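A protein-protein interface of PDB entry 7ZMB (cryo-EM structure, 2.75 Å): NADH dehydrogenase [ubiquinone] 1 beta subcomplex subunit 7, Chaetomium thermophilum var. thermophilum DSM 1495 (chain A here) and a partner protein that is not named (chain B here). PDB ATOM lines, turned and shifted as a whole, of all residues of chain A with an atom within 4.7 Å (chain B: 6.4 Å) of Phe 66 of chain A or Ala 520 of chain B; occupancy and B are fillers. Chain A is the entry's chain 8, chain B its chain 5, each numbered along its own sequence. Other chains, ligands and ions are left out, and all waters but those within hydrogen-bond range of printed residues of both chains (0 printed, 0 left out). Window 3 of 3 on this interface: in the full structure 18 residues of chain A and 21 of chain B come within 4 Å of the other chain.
Among the printed residues, pairs that only touch across the chains: Arg 69 of chain A with Ile 515 of chain B (3.2 Å), Gln 62 of chain A with Ile 515 of chain B (3.4 Å), Tyr 63 of chain A with Phe 519 of chain B (3.5 Å), Phe 66 of chain A with Ala 520 of chain B (3.6 Å) and Phe 66 of chain A with Phe 519 of chain B (3.6 Å).
Of chain B, only Phe 519 and Ala 520 come within 4 Å of Phe 66 of chain A. Of the printed residues of chain A, Phe 519 of chain B touches Tyr 63 and Phe 66. Printed residues of chain B within 4 Å of Arg 69 of chain A: Ile 515 (3.2 Å). Of the printed residues of chain B, Gln 62 of chain A touches Ile 515 (3.4 Å). Of the printed residues of chain A, Ile 515 of chain B touches Gln 62 (3.4 Å) and Arg 69 (3.2 Å). Val 521 of chain B touches none of the printed residues of chain A. Val 70 of chain A touches none of the printed residues of chain B. The nearest printed residue of chain A that does not touch Ala 520 of chain B is Val 70 of chain A (7.1 Å). The nearest printed residue of chain A that does not touch Phe 519 of chain B is Gln 62 of chain A (4.03 Å).
Of the 9 printed residues of chain A, 4 touch a printed residue of chain B. Printed residues of chain A that touch a printed residue of chain B: Gln 62, Tyr 63, Phe 66 and Arg 69. Of the 11 printed residues of chain B, 3 touch a printed residue of chain A. Among the printed residues, no Asp or Glu carboxylate lies within 4 Å of a Lys or Arg side-chain nitrogen of the other chain.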
ATOM      1  N   GLN A  62      20.274   4.085 -20.320  1.00  0.00           N
ATOM      2  CA  GLN A  62      20.487   2.710 -19.881  1.00  0.00           C
ATOM      3  C   GLN A  62      21.822   2.567 -19.158  1.00  0.00           C
ATOM      4  O   GLN A  62      21.904   1.934 -18.100  1.00  0.00           O
ATOM      5  CB  GLN A  62      20.418   1.762 -21.077  1.00  0.00           C
ATOM      6  CG  GLN A  62      19.033   1.622 -21.684  1.00  0.00           C
ATOM      7  CD  GLN A  62      18.062   0.907 -20.767  1.00  0.00           C
ATOM      8  OE1 GLN A  62      18.172  -0.299 -20.547  1.00  0.00           O
ATOM      9  NE2 GLN A  62      17.102   1.648 -20.229  1.00  0.00           N
ATOM     10  N   TYR A  63      22.883   3.154 -19.718  1.00  0.00           N
ATOM     11  CA  TYR A  63      24.197   3.058 -19.091  1.00  0.00           C
ATOM     12  C   TYR A  63      24.232   3.796 -17.760  1.00  0.00           C
ATOM     13  O   TYR A  63      24.777   3.284 -16.775  1.00  0.00           O
ATOM     14  CB  TYR A  63      25.268   3.598 -20.035  1.00  0.00           C
ATOM     15  CG  TYR A  63      26.677   3.502 -19.504  1.00  0.00           C
ATOM     16  CD1 TYR A  63      27.352   2.290 -19.481  1.00  0.00           C
ATOM     17  CD2 TYR A  63      27.337   4.628 -19.030  1.00  0.00           C
ATOM     18  CE1 TYR A  63      28.643   2.201 -18.999  1.00  0.00           C
ATOM     19  CE2 TYR A  63      28.627   4.548 -18.547  1.00  0.00           C
ATOM     20  CZ  TYR A  63      29.275   3.333 -18.533  1.00  0.00           C
ATOM     21  OH  TYR A  63      30.561   3.251 -18.052  1.00  0.00           O
ATOM     22  N   LEU A  64      23.659   5.000 -17.710  1.00  0.00           N
ATOM     23  CA  LEU A  64      23.610   5.740 -16.454  1.00  0.00           C
ATOM     24  C   LEU A  64      22.779   4.999 -15.415  1.00  0.00           C
ATOM     25  O   LEU A  64      23.143   4.954 -14.234  1.00  0.00           O
ATOM     26  CB  LEU A  64      23.053   7.143 -16.689  1.00  0.00           C
ATOM     27  CG  LEU A  64      23.913   8.072 -17.546  1.00  0.00           C
ATOM     28  CD1 LEU A  64      23.184   9.377 -17.816  1.00  0.00           C
ATOM     29  CD2 LEU A  64      25.253   8.330 -16.880  1.00  0.00           C
ATOM     30  N   GLU A  65      21.655   4.416 -15.837  1.00  0.00           N
ATOM     31  CA  GLU A  65      20.849   3.617 -14.921  1.00  0.00           C
ATOM     32  C   GLU A  65      21.619   2.395 -14.435  1.00  0.00           C
ATOM     33  O   GLU A  65      21.544   2.035 -13.255  1.00  0.00           O
ATOM     34  CB  GLU A  65      19.547   3.191 -15.598  1.00  0.00           C
ATOM     35  CG  GLU A  65      18.618   2.385 -14.707  1.00  0.00           C
ATOM     36  CD  GLU A  65      18.097   3.185 -13.531  1.00  0.00           C
ATOM     37  OE1 GLU A  65      18.029   4.428 -13.636  1.00  0.00           O
ATOM     38  OE2 GLU A  65      17.753   2.570 -12.500  1.00  0.00           O
ATOM     39  N   PHE A  66      22.373   1.755 -15.330  1.00  0.00           N
ATOM     40  CA  PHE A  66      23.097   0.542 -14.962  1.00  0.00           C
ATOM     41  C   PHE A  66      24.100   0.808 -13.847  1.00  0.00           C
ATOM     42  O   PHE A  66      24.213   0.016 -12.904  1.00  0.00           O
ATOM     43  CB  PHE A  66      23.802  -0.034 -16.189  1.00  0.00           C
ATOM     44  CG  PHE A  66      24.568  -1.292 -15.911  1.00  0.00           C
ATOM     45  CD1 PHE A  66      23.976  -2.343 -15.235  1.00  0.00           C
ATOM     46  CD2 PHE A  66      25.884  -1.421 -16.321  1.00  0.00           C
ATOM     47  CE1 PHE A  66      24.681  -3.501 -14.977  1.00  0.00           C
ATOM     48  CE2 PHE A  66      26.595  -2.576 -16.064  1.00  0.00           C
ATOM     49  CZ  PHE A  66      25.992  -3.617 -15.392  1.00  0.00           C
ATOM     50  N   LYS A  67      24.839   1.916 -13.936  1.00  0.00           N
ATOM     51  CA  LYS A  67      25.819   2.227 -12.900  1.00  0.00           C
ATOM     52  C   LYS A  67      25.146   2.508 -11.564  1.00  0.00           C
ATOM     53  O   LYS A  67      25.647   2.096 -10.512  1.00  0.00           O
ATOM     54  CB  LYS A  67      26.690   3.403 -13.333  1.00  0.00           C
ATOM     55  CG  LYS A  67      27.493   3.114 -14.583  1.00  0.00           C
ATOM     56  CD  LYS A  67      28.537   2.045 -14.297  1.00  0.00           C
ATOM     57  CE  LYS A  67      29.413   1.780 -15.504  1.00  0.00           C
ATOM     58  NZ  LYS A  67      30.409   0.706 -15.246  1.00  0.00           N
ATOM     59  N   LYS A  68      24.011   3.208 -11.581  1.00  0.00           N
ATOM     60  CA  LYS A  68      23.253   3.401 -10.349  1.00  0.00           C
ATOM     61  C   LYS A  68      22.790   2.066  -9.784  1.00  0.00           C
ATOM     62  O   LYS A  68      22.771   1.868  -8.564  1.00  0.00           O
ATOM     63  CB  LYS A  68      22.058   4.319 -10.606  1.00  0.00           C
ATOM     64  CG  LYS A  68      22.431   5.755 -10.934  1.00  0.00           C
ATOM     65  CD  LYS A  68      21.190   6.610 -11.125  1.00  0.00           C
ATOM     66  CE  LYS A  68      21.552   8.048 -11.457  1.00  0.00           C
ATOM     67  NZ  LYS A  68      20.337   8.888 -11.647  1.00  0.00           N
ATOM     68  N   ARG A  69      22.411   1.139 -10.663  1.00  0.00           N
ATOM     69  CA  ARG A  69      21.963  -0.180 -10.231  1.00  0.00           C
ATOM     70  C   ARG A  69      23.107  -0.995  -9.638  1.00  0.00           C
ATOM     71  O   ARG A  69      22.976  -1.562  -8.547  1.00  0.00           O
ATOM     72  CB  ARG A  69      21.329  -0.907 -11.416  1.00  0.00           C
ATOM     73  CG  ARG A  69      20.038  -0.267 -11.893  1.00  0.00           C
ATOM     74  CD  ARG A  69      19.471  -0.997 -13.089  1.00  0.00           C
ATOM     75  NE  ARG A  69      19.034  -2.349 -12.780  1.00  0.00           N
ATOM     76  CZ  ARG A  69      18.655  -3.224 -13.703  1.00  0.00           C
ATOM     77  NH1 ARG A  69      18.278  -4.442 -13.355  1.00  0.00           N
ATOM     78  NH2 ARG A  69      18.654  -2.874 -14.980  1.00  0.00           N
ATOM     79  N   VAL A  70      24.241  -1.063 -10.340  1.00  0.00           N
ATOM     80  CA  VAL A  70      25.349  -1.883  -9.858  1.00  0.00           C
ATOM     81  C   VAL A  70      25.956  -1.288  -8.593  1.00  0.00           C
ATOM     82  O   VAL A  70      26.400  -2.025  -7.704  1.00  0.00           O
ATOM     83  CB  VAL A  70      26.403  -2.078 -10.964  1.00  0.00           C
ATOM     84  CG1 VAL A  70      27.026  -0.756 -11.365  1.00  0.00           C
ATOM     85  CG2 VAL A  70      27.473  -3.059 -10.513  1.00  0.00           C
ATOM     86  N   TYR B 400      26.360 -15.902 -20.931  1.00  0.00           N
ATOM     87  CA  TYR B 400      27.031 -15.374 -19.752  1.00  0.00           C
ATOM     88  C   TYR B 400      26.290 -14.186 -19.155  1.00  0.00           C
ATOM     89  O   TYR B 400      26.410 -13.929 -17.953  1.00  0.00           O
ATOM     90  CB  TYR B 400      28.466 -14.976 -20.092  1.00  0.00           C
ATOM     91  CG  TYR B 400      29.297 -14.604 -18.887  1.00  0.00           C
ATOM     92  CD1 TYR B 400      29.898 -15.582 -18.104  1.00  0.00           C
ATOM     93  CD2 TYR B 400      29.480 -13.277 -18.530  1.00  0.00           C
ATOM     94  CE1 TYR B 400      30.655 -15.244 -17.002  1.00  0.00           C
ATOM     95  CE2 TYR B 400      30.235 -12.931 -17.431  1.00  0.00           C
ATOM     96  CZ  TYR B 400      30.820 -13.917 -16.670  1.00  0.00           C
ATOM     97  OH  TYR B 400      31.575 -13.569 -15.576  1.00  0.00           O
ATOM     98  N   GLY B 401      25.528 -13.454 -19.972  1.00  0.00           N
ATOM     99  CA  GLY B 401      24.791 -12.313 -19.454  1.00  0.00           C
ATOM    100  C   GLY B 401      23.782 -12.706 -18.394  1.00  0.00           C
ATOM    101  O   GLY B 401      23.589 -11.989 -17.410  1.00  0.00           O
ATOM    102  N   PHE B 403      23.339 -13.987 -15.395  1.00  0.00           N
ATOM    103  CA  PHE B 403      24.277 -14.264 -14.310  1.00  0.00           C
ATOM    104  C   PHE B 403      23.655 -15.283 -13.361  1.00  0.00           C
ATOM    105  O   PHE B 403      23.227 -14.976 -12.246  1.00  0.00           O
ATOM    106  CB  PHE B 403      24.658 -12.978 -13.592  1.00  0.00           C
ATOM    107  CG  PHE B 403      25.738 -12.203 -14.287  1.00  0.00           C
ATOM    108  CD1 PHE B 403      27.053 -12.631 -14.239  1.00  0.00           C
ATOM    109  CD2 PHE B 403      25.436 -11.056 -14.998  1.00  0.00           C
ATOM    110  CE1 PHE B 403      28.048 -11.925 -14.882  1.00  0.00           C
ATOM    111  CE2 PHE B 403      26.428 -10.346 -15.644  1.00  0.00           C
ATOM    112  CZ  PHE B 403      27.735 -10.780 -15.585  1.00  0.00           C
ATOM    113  N   ILE B 515      20.298  -6.131 -21.675  1.00  0.00           N
ATOM    114  CA  ILE B 515      21.141  -5.050 -21.172  1.00  0.00           C
ATOM    115  C   ILE B 515      22.391  -5.606 -20.501  1.00  0.00           C
ATOM    116  O   ILE B 515      23.480  -5.032 -20.617  1.00  0.00           O
ATOM    117  CB  ILE B 515      20.338  -4.136 -20.229  1.00  0.00           C
ATOM    118  CG1 ILE B 515      19.844  -4.913 -19.007  1.00  0.00           C
ATOM    119  CG2 ILE B 515      19.173  -3.499 -20.965  1.00  0.00           C
ATOM    120  CD1 ILE B 515      19.256  -4.037 -17.940  1.00  0.00           C
ATOM    121  N   ASP B 516      22.260  -6.727 -19.789  1.00  0.00           N
ATOM    122  CA  ASP B 516      23.421  -7.342 -19.160  1.00  0.00           C
ATOM    123  C   ASP B 516      24.357  -7.973 -20.177  1.00  0.00           C
ATOM    124  O   ASP B 516      25.552  -8.120 -19.896  1.00  0.00           O
ATOM    125  CB  ASP B 516      22.975  -8.390 -18.143  1.00  0.00           C
ATOM    126  CG  ASP B 516      22.301  -7.777 -16.935  1.00  0.00           C
ATOM    127  OD1 ASP B 516      22.635  -6.626 -16.589  1.00  0.00           O
ATOM    128  OD2 ASP B 516      21.437  -8.446 -16.330  1.00  0.00           O
ATOM    129  N   THR B 517      23.842  -8.349 -21.349  1.00  0.00           N
ATOM    130  CA  THR B 517      24.684  -8.945 -22.379  1.00  0.00           C
ATOM    131  C   THR B 517      25.718  -7.956 -22.902  1.00  0.00           C
ATOM    132  O   THR B 517      26.819  -8.360 -23.294  1.00  0.00           O
ATOM    133  CB  THR B 517      23.814  -9.461 -23.526  1.00  0.00           C
ATOM    134  OG1 THR B 517      22.773 -10.295 -23.001  1.00  0.00           O
ATOM    135  CG2 THR B 517      24.642 -10.263 -24.515  1.00  0.00           C
ATOM    136  N   GLU B 518      25.390  -6.666 -22.908  1.00  0.00           N
ATOM    137  CA  GLU B 518      26.271  -5.654 -23.474  1.00  0.00           C
ATOM    138  C   GLU B 518      27.101  -4.918 -22.431  1.00  0.00           C
ATOM    139  O   GLU B 518      28.176  -4.410 -22.768  1.00  0.00           O
ATOM    140  CB  GLU B 518      25.446  -4.633 -24.273  1.00  0.00           C
ATOM    141  CG  GLU B 518      26.267  -3.658 -25.102  1.00  0.00           C
ATOM    142  CD  GLU B 518      25.551  -3.222 -26.366  1.00  0.00           C
ATOM    143  OE1 GLU B 518      24.748  -4.016 -26.899  1.00  0.00           O
ATOM    144  OE2 GLU B 518      25.789  -2.086 -26.826  1.00  0.00           O
ATOM    145  N   PHE B 519      26.645  -4.859 -21.180  1.00  0.00           N
ATOM    146  CA  PHE B 519      27.255  -3.998 -20.173  1.00  0.00           C
ATOM    147  C   PHE B 519      27.958  -4.780 -19.071  1.00  0.00           C
ATOM    148  O   PHE B 519      29.150  -4.576 -18.831  1.00  0.00           O
ATOM    149  CB  PHE B 519      26.186  -3.078 -19.565  1.00  0.00           C
ATOM    150  CG  PHE B 519      25.760  -1.954 -20.469  1.00  0.00           C
ATOM    151  CD1 PHE B 519      26.232  -1.864 -21.767  1.00  0.00           C
ATOM    152  CD2 PHE B 519      24.874  -0.992 -20.019  1.00  0.00           C
ATOM    153  CE1 PHE B 519      25.838  -0.835 -22.594  1.00  0.00           C
ATOM    154  CE2 PHE B 519      24.474   0.039 -20.843  1.00  0.00           C
ATOM    155  CZ  PHE B 519      24.957   0.118 -22.130  1.00  0.00           C
ATOM    156  N   ALA B 520      27.246  -5.679 -18.390  1.00  0.00           N
ATOM    157  CA  ALA B 520      27.795  -6.299 -17.189  1.00  0.00           C
ATOM    158  C   ALA B 520      28.886  -7.312 -17.507  1.00  0.00           C
ATOM    159  O   ALA B 520      29.749  -7.573 -16.661  1.00  0.00           O
ATOM    160  CB  ALA B 520      26.678  -6.961 -16.385  1.00  0.00           C
ATOM    161  N   VAL B 521      28.865  -7.894 -18.702  1.00  0.00           N
ATOM    162  CA  VAL B 521      29.874  -8.901 -19.047  1.00  0.00           C
ATOM    163  C   VAL B 521      31.248  -8.243 -19.091  1.00  0.00           C
ATOM    164  O   VAL B 521      31.379  -7.115 -19.607  1.00  0.00           O
ATOM    165  CB  VAL B 521      29.529  -9.571 -20.390  1.00  0.00           C
ATOM    166  CG1 VAL B 521      29.468  -8.545 -21.509  1.00  0.00           C
ATOM    167  CG2 VAL B 521      30.526 -10.665 -20.727  1.00  0.00           C
ATOM    168  N   PRO B 522      32.290  -8.860 -18.540  1.00  0.00           N
ATOM    169  CA  PRO B 522      33.632  -8.282 -18.665  1.00  0.00           C
ATOM    170  C   PRO B 522      34.131  -8.343 -20.099  1.00  0.00           C
ATOM    171  O   PRO B 522      33.715  -9.187 -20.895  1.00  0.00           O
ATOM    172  CB  PRO B 522      34.482  -9.152 -17.736  1.00  0.00           C
ATOM    173  CG  PRO B 522      33.775 -10.458 -17.703  1.00  0.00           C
ATOM    174  CD  PRO B 522      32.308 -10.130 -17.793  1.00  0.00           C
